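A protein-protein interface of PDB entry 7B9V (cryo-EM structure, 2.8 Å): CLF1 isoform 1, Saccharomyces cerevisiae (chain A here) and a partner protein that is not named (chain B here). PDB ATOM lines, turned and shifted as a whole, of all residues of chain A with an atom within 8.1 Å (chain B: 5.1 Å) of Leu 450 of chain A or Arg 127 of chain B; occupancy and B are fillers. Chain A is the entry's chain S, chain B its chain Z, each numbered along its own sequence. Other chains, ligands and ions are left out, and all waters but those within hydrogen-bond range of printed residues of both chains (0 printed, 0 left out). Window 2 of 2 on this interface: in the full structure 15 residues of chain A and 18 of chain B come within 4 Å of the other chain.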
ATOM      1  N   ALA A 411      35.094   2.607 -10.309  1.00  0.00           N
ATOM      2  CA  ALA A 411      34.307   1.743 -11.192  1.00  0.00           C
ATOM      3  C   ALA A 411      33.333   2.530 -12.065  1.00  0.00           C
ATOM      4  O   ALA A 411      33.235   2.279 -13.271  1.00  0.00           O
ATOM      5  CB  ALA A 411      33.551   0.706 -10.367  1.00  0.00           C
ATOM      6  N   ILE A 415      33.765   4.017 -16.719  1.00  0.00           N
ATOM      7  CA  ILE A 415      32.744   4.077 -17.762  1.00  0.00           C
ATOM      8  C   ILE A 415      32.825   5.405 -18.517  1.00  0.00           C
ATOM      9  O   ILE A 415      32.770   5.438 -19.755  1.00  0.00           O
ATOM     10  CB  ILE A 415      31.351   3.837 -17.144  1.00  0.00           C
ATOM     11  CG1 ILE A 415      31.332   2.475 -16.445  1.00  0.00           C
ATOM     12  CG2 ILE A 415      30.254   3.919 -18.191  1.00  0.00           C
ATOM     13  CD1 ILE A 415      30.074   2.190 -15.666  1.00  0.00           C
ATOM     14  N   VAL A 420      35.688   1.872 -20.398  1.00  0.00           N
ATOM     15  CA  VAL A 420      34.593   1.167 -19.708  1.00  0.00           C
ATOM     16  C   VAL A 420      34.870  -0.329 -19.299  1.00  0.00           C
ATOM     17  O   VAL A 420      34.526  -0.656 -18.165  1.00  0.00           O
ATOM     18  CB  VAL A 420      33.272   1.326 -20.524  1.00  0.00           C
ATOM     19  N   PRO A 421      35.423  -1.222 -20.160  1.00  0.00           N
ATOM     20  CA  PRO A 421      35.701  -2.615 -19.715  1.00  0.00           C
ATOM     21  C   PRO A 421      36.668  -2.765 -18.534  1.00  0.00           C
ATOM     22  O   PRO A 421      36.662  -3.809 -17.877  1.00  0.00           O
ATOM     23  CB  PRO A 421      36.265  -3.312 -20.965  1.00  0.00           C
ATOM     24  CG  PRO A 421      35.684  -2.624 -22.068  1.00  0.00           C
ATOM     25  CD  PRO A 421      35.656  -1.178 -21.618  1.00  0.00           C
ATOM     26  N   ALA A 423      36.533  -1.480 -15.615  1.00  0.00           N
ATOM     27  CA  ALA A 423      35.806  -1.498 -14.336  1.00  0.00           C
ATOM     28  C   ALA A 423      35.674  -2.892 -13.706  1.00  0.00           C
ATOM     29  O   ALA A 423      35.266  -2.986 -12.543  1.00  0.00           O
ATOM     30  CB  ALA A 423      34.405  -0.904 -14.519  1.00  0.00           C
ATOM     31  N   ARG A 424      36.016  -3.957 -14.433  1.00  0.00           N
ATOM     32  CA  ARG A 424      36.015  -5.321 -13.909  1.00  0.00           C
ATOM     33  C   ARG A 424      37.184  -5.549 -12.955  1.00  0.00           C
ATOM     34  O   ARG A 424      37.009  -6.164 -11.894  1.00  0.00           O
ATOM     35  CB  ARG A 424      36.073  -6.326 -15.054  1.00  0.00           C
ATOM     36  N   TYR A 443      28.475  -3.134  -6.949  1.00  0.00           N
ATOM     37  CA  TYR A 443      28.870  -3.771  -8.205  1.00  0.00           C
ATOM     38  C   TYR A 443      27.707  -4.503  -8.859  1.00  0.00           C
ATOM     39  O   TYR A 443      27.600  -4.515 -10.093  1.00  0.00           O
ATOM     40  CB  TYR A 443      30.053  -4.721  -7.998  1.00  0.00           C
ATOM     41  CG  TYR A 443      30.457  -5.425  -9.282  1.00  0.00           C
ATOM     42  CD1 TYR A 443      31.221  -4.768 -10.235  1.00  0.00           C
ATOM     43  CD2 TYR A 443      30.126  -6.765  -9.510  1.00  0.00           C
ATOM     44  CE1 TYR A 443      31.601  -5.396 -11.405  1.00  0.00           C
ATOM     45  CE2 TYR A 443      30.505  -7.405 -10.677  1.00  0.00           C
ATOM     46  CZ  TYR A 443      31.244  -6.715 -11.617  1.00  0.00           C
ATOM     47  OH  TYR A 443      31.622  -7.344 -12.779  1.00  0.00           O
ATOM     48  N   ILE A 444      26.847  -5.138  -8.052  1.00  0.00           N
ATOM     49  CA  ILE A 444      25.708  -5.861  -8.613  1.00  0.00           C
ATOM     50  C   ILE A 444      24.718  -4.882  -9.232  1.00  0.00           C
ATOM     51  O   ILE A 444      24.193  -5.134 -10.326  1.00  0.00           O
ATOM     52  CB  ILE A 444      25.061  -6.787  -7.556  1.00  0.00           C
ATOM     53  CG1 ILE A 444      25.990  -7.945  -7.186  1.00  0.00           C
ATOM     54  CG2 ILE A 444      23.717  -7.364  -7.995  1.00  0.00           C
ATOM     55  CD1 ILE A 444      25.667  -8.579  -5.854  1.00  0.00           C
ATOM     56  N   GLU A 445      24.491  -3.730  -8.569  1.00  0.00           N
ATOM     57  CA  GLU A 445      23.633  -2.699  -9.159  1.00  0.00           C
ATOM     58  C   GLU A 445      24.241  -2.139 -10.445  1.00  0.00           C
ATOM     59  O   GLU A 445      23.511  -1.850 -11.404  1.00  0.00           O
ATOM     60  CB  GLU A 445      23.367  -1.577  -8.151  1.00  0.00           C
ATOM     61  CG  GLU A 445      22.414  -0.505  -8.676  1.00  0.00           C
ATOM     62  CD  GLU A 445      21.971   0.473  -7.623  1.00  0.00           C
ATOM     63  OE1 GLU A 445      22.821   1.249  -7.139  1.00  0.00           O
ATOM     64  OE2 GLU A 445      20.771   0.462  -7.282  1.00  0.00           O
ATOM     65  N   LEU A 446      25.580  -1.983 -10.479  1.00  0.00           N
ATOM     66  CA  LEU A 446      26.235  -1.490 -11.690  1.00  0.00           C
ATOM     67  C   LEU A 446      26.086  -2.480 -12.836  1.00  0.00           C
ATOM     68  O   LEU A 446      25.909  -2.069 -13.988  1.00  0.00           O
ATOM     69  CB  LEU A 446      27.713  -1.205 -11.422  1.00  0.00           C
ATOM     70  CG  LEU A 446      28.474  -0.499 -12.548  1.00  0.00           C
ATOM     71  CD1 LEU A 446      27.932   0.896 -12.791  1.00  0.00           C
ATOM     72  CD2 LEU A 446      29.957  -0.444 -12.220  1.00  0.00           C
ATOM     73  N   GLU A 447      26.205  -3.784 -12.537  1.00  0.00           N
ATOM     74  CA  GLU A 447      25.919  -4.833 -13.515  1.00  0.00           C
ATOM     75  C   GLU A 447      24.495  -4.737 -14.041  1.00  0.00           C
ATOM     76  O   GLU A 447      24.260  -4.878 -15.245  1.00  0.00           O
ATOM     77  CB  GLU A 447      26.168  -6.212 -12.912  1.00  0.00           C
ATOM     78  CG  GLU A 447      27.625  -6.596 -12.715  1.00  0.00           C
ATOM     79  CD  GLU A 447      28.261  -7.258 -13.941  1.00  0.00           C
ATOM     80  OE1 GLU A 447      27.867  -6.977 -15.095  1.00  0.00           O
ATOM     81  OE2 GLU A 447      29.176  -8.081 -13.734  1.00  0.00           O
ATOM     82  N   VAL A 448      23.533  -4.538 -13.124  1.00  0.00           N
ATOM     83  CA  VAL A 448      22.114  -4.485 -13.481  1.00  0.00           C
ATOM     84  C   VAL A 448      21.843  -3.287 -14.387  1.00  0.00           C
ATOM     85  O   VAL A 448      21.094  -3.388 -15.370  1.00  0.00           O
ATOM     86  CB  VAL A 448      21.256  -4.477 -12.193  1.00  0.00           C
ATOM     87  CG1 VAL A 448      19.813  -4.060 -12.443  1.00  0.00           C
ATOM     88  CG2 VAL A 448      21.241  -5.872 -11.572  1.00  0.00           C
ATOM     89  N   LYS A 449      22.514  -2.159 -14.113  1.00  0.00           N
ATOM     90  CA  LYS A 449      22.397  -0.983 -14.967  1.00  0.00           C
ATOM     91  C   LYS A 449      23.069  -1.211 -16.316  1.00  0.00           C
ATOM     92  O   LYS A 449      22.563  -0.770 -17.353  1.00  0.00           O
ATOM     93  CB  LYS A 449      22.973   0.247 -14.260  1.00  0.00           C
ATOM     94  CG  LYS A 449      22.123   0.712 -13.084  1.00  0.00           C
ATOM     95  CD  LYS A 449      22.541   2.081 -12.573  1.00  0.00           C
ATOM     96  CE  LYS A 449      21.868   2.392 -11.245  1.00  0.00           C
ATOM     97  NZ  LYS A 449      21.852   3.851 -10.942  1.00  0.00           N
ATOM     98  N   LEU A 450      24.200  -1.916 -16.322  1.00  0.00           N
ATOM     99  CA  LEU A 450      24.877  -2.279 -17.564  1.00  0.00           C
ATOM    100  C   LEU A 450      24.147  -3.426 -18.254  1.00  0.00           C
ATOM    101  O   LEU A 450      24.464  -3.780 -19.388  1.00  0.00           O
ATOM    102  CB  LEU A 450      26.346  -2.643 -17.309  1.00  0.00           C
ATOM    103  CG  LEU A 450      27.279  -1.493 -16.906  1.00  0.00           C
ATOM    104  CD1 LEU A 450      28.517  -2.022 -16.200  1.00  0.00           C
ATOM    105  CD2 LEU A 450      27.665  -0.662 -18.118  1.00  0.00           C
ATOM    106  N   PHE A 453      25.576  -8.016 -18.419  1.00  0.00           N
ATOM    107  CA  PHE A 453      24.794  -7.626 -17.254  1.00  0.00           C
ATOM    108  C   PHE A 453      24.417  -8.822 -16.391  1.00  0.00           C
ATOM    109  O   PHE A 453      24.154  -8.684 -15.196  1.00  0.00           O
ATOM    110  CB  PHE A 453      23.522  -6.911 -17.703  1.00  0.00           C
ATOM    111  N   ASP A 454      24.400 -10.004 -17.006  1.00  0.00           N
ATOM    112  CA  ASP A 454      23.943 -11.205 -16.323  1.00  0.00           C
ATOM    113  C   ASP A 454      24.973 -11.799 -15.376  1.00  0.00           C
ATOM    114  O   ASP A 454      24.614 -12.684 -14.591  1.00  0.00           O
ATOM    115  CB  ASP A 454      23.532 -12.269 -17.341  1.00  0.00           C
ATOM    116  N   ILE B 120      26.305   4.923 -19.730  1.00  0.00           N
ATOM    117  CA  ILE B 120      25.933   3.508 -19.695  1.00  0.00           C
ATOM    118  C   ILE B 120      24.928   3.212 -20.797  1.00  0.00           C
ATOM    119  O   ILE B 120      25.049   2.216 -21.520  1.00  0.00           O
ATOM    120  CB  ILE B 120      25.420   3.113 -18.293  1.00  0.00           C
ATOM    121  CG1 ILE B 120      26.594   2.924 -17.331  1.00  0.00           C
ATOM    122  CG2 ILE B 120      24.551   1.856 -18.310  1.00  0.00           C
ATOM    123  CD1 ILE B 120      26.166   2.738 -15.901  1.00  0.00           C
ATOM    124  N   ILE B 123      26.804   3.165 -24.217  1.00  0.00           N
ATOM    125  CA  ILE B 123      27.494   1.909 -24.543  1.00  0.00           C
ATOM    126  C   ILE B 123      26.492   0.758 -24.752  1.00  0.00           C
ATOM    127  O   ILE B 123      26.753  -0.148 -25.559  1.00  0.00           O
ATOM    128  CB  ILE B 123      28.626   1.583 -23.527  1.00  0.00           C
ATOM    129  CG1 ILE B 123      29.499   0.416 -24.032  1.00  0.00           C
ATOM    130  CG2 ILE B 123      28.111   1.260 -22.150  1.00  0.00           C
ATOM    131  CD1 ILE B 123      30.835   0.249 -23.366  1.00  0.00           C
ATOM    132  N   ILE B 124      25.320   0.790 -24.082  1.00  0.00           N
ATOM    133  CA  ILE B 124      24.293  -0.225 -24.356  1.00  0.00           C
ATOM    134  C   ILE B 124      23.755  -0.061 -25.777  1.00  0.00           C
ATOM    135  O   ILE B 124      23.572  -1.057 -26.498  1.00  0.00           O
ATOM    136  CB  ILE B 124      23.171  -0.191 -23.290  1.00  0.00           C
ATOM    137  CG1 ILE B 124      23.672  -0.692 -21.940  1.00  0.00           C
ATOM    138  CG2 ILE B 124      21.939  -1.013 -23.671  1.00  0.00           C
ATOM    139  CD1 ILE B 124      22.770  -0.288 -20.808  1.00  0.00           C
ATOM    140  N   ARG B 125      23.489   1.191 -26.198  1.00  0.00           N
ATOM    141  CA  ARG B 125      23.008   1.458 -27.553  1.00  0.00           C
ATOM    142  C   ARG B 125      24.051   1.055 -28.593  1.00  0.00           C
ATOM    143  O   ARG B 125      23.701   0.729 -29.730  1.00  0.00           O
ATOM    144  CB  ARG B 125      22.632   2.936 -27.702  1.00  0.00           C
ATOM    145  CG  ARG B 125      21.362   3.334 -26.956  1.00  0.00           C
ATOM    146  CD  ARG B 125      21.288   4.838 -26.781  1.00  0.00           C
ATOM    147  NE  ARG B 125      20.167   5.223 -25.934  1.00  0.00           N
ATOM    148  CZ  ARG B 125      19.870   6.472 -25.602  1.00  0.00           C
ATOM    149  NH1 ARG B 125      20.595   7.491 -26.033  1.00  0.00           N
ATOM    150  NH2 ARG B 125      18.832   6.702 -24.805  1.00  0.00           N
ATOM    151  N   LYS B 126      25.344   1.152 -28.246  1.00  0.00           N
ATOM    152  CA  LYS B 126      26.363   0.647 -29.160  1.00  0.00           C
ATOM    153  C   LYS B 126      26.383  -0.882 -29.196  1.00  0.00           C
ATOM    154  O   LYS B 126      26.635  -1.472 -30.255  1.00  0.00           O
ATOM    155  CB  LYS B 126      27.742   1.182 -28.780  1.00  0.00           C
ATOM    156  CG  LYS B 126      28.761   1.035 -29.902  1.00  0.00           C
ATOM    157  CD  LYS B 126      30.090   1.664 -29.555  1.00  0.00           C
ATOM    158  CE  LYS B 126      31.092   1.472 -30.682  1.00  0.00           C
ATOM    159  NZ  LYS B 126      30.751   2.263 -31.895  1.00  0.00           N
ATOM    160  N   ARG B 127      26.154  -1.535 -28.039  1.00  0.00           N
ATOM    161  CA  ARG B 127      26.247  -2.998 -27.954  1.00  0.00           C
ATOM    162  C   ARG B 127      25.174  -3.701 -28.777  1.00  0.00           C
ATOM    163  O   ARG B 127      25.426  -4.778 -29.330  1.00  0.00           O
ATOM    164  CB  ARG B 127      26.182  -3.470 -26.500  1.00  0.00           C
ATOM    165  CG  ARG B 127      27.507  -3.365 -25.749  1.00  0.00           C
ATOM    166  CD  ARG B 127      27.293  -3.362 -24.251  1.00  0.00           C
ATOM    167  NE  ARG B 127      26.595  -4.561 -23.805  1.00  0.00           N
ATOM    168  CZ  ARG B 127      26.032  -4.700 -22.613  1.00  0.00           C
ATOM    169  NH1 ARG B 127      26.059  -3.725 -21.719  1.00  0.00           N
ATOM    170  NH2 ARG B 127      25.437  -5.850 -22.307  1.00  0.00           N
ATOM    171  N   VAL B 128      23.985  -3.111 -28.876  1.00  0.00           N
ATOM    172  CA  VAL B 128      22.892  -3.721 -29.630  1.00  0.00           C
ATOM    173  C   VAL B 128      23.098  -3.625 -31.149  1.00  0.00           C
ATOM    174  O   VAL B 128      24.164  -3.248 -31.645  1.00  0.00           O
ATOM    175  CB  VAL B 128      21.508  -3.131 -29.221  1.00  0.00           C
ATOM    176  CG1 VAL B 128      21.171  -3.486 -27.769  1.00  0.00           C
ATOM    177  CG2 VAL B 128      21.439  -1.638 -29.451  1.00  0.00           C
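CG1 of Ile 120 of chain B touches CG2 of Ile 415 of chain A, at 3.9 Å.
Ile 123 of chain B touches Val 420 of chain A.
Ile 120 of chain B touches Lys 449 of chain A (CG2 to O, 3.4 Å).
Lys 449 of chain A touches Ile 124 of chain B (O to CD1, 3.5 Å).
Leu 450 of chain A touches Ile 120 of chain B (CD2 to CG1, 3.8 Å).
Of chain B, only Ile 120 (3.8 Å) and Arg 127 (2.8 Å) come within 4 Å of Leu 450 of chain A.
Printed residues of chain A within 4 Å of Arg 127 of chain B: Leu 450 (2.8 Å).
Of the printed residues of chain A, Ile 120 of chain B touches Ile 415 (3.9 Å), Lys 449 (3.4 Å) and Leu 450 (3.8 Å).
Printed residues of chain A within 4 Å of Ile 124 of chain B: Lys 449 (3.5 Å).
Of the printed residues of chain B, Val 420 of chain A touches Ile 123 (3.9 Å).
Of the printed residues of chain A, Ile 123 of chain B touches Val 420 (3.9 Å).
Of the printed residues of chain B, Ile 415 of chain A touches Ile 120.
Pro 421 of chain A touches none of the printed residues of chain B.
Phe 453 of chain A touches none of the printed residues of chain B.
The nearest residue of chain A that does not touch Arg 127 of chain B is Phe 453 of chain A (4.5 Å).
Printed residues of chain A that touch a printed residue of chain B: Ile 415, Val 420, Lys 449 and Leu 450.
Hydrophobic or aromatic side chains of chain A within 4 Å of the printed part of chain B: Ile 415, Val 420 and Leu 450.
Hydrophobic or aromatic side chains of chain B within 4 Å of the printed part of chain A: Ile 120, Ile 123 and Ile 124.
Along chain B the printed residues that touch a printed residue of chain A span positions 120 to 127.
Among the printed residues, 6 pairs touch across the chains.
The guanidinium group of Arg 127 of chain B is in hydrogen-bond range of the backbone carbonyl oxygen of Leu 450 of chain A.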
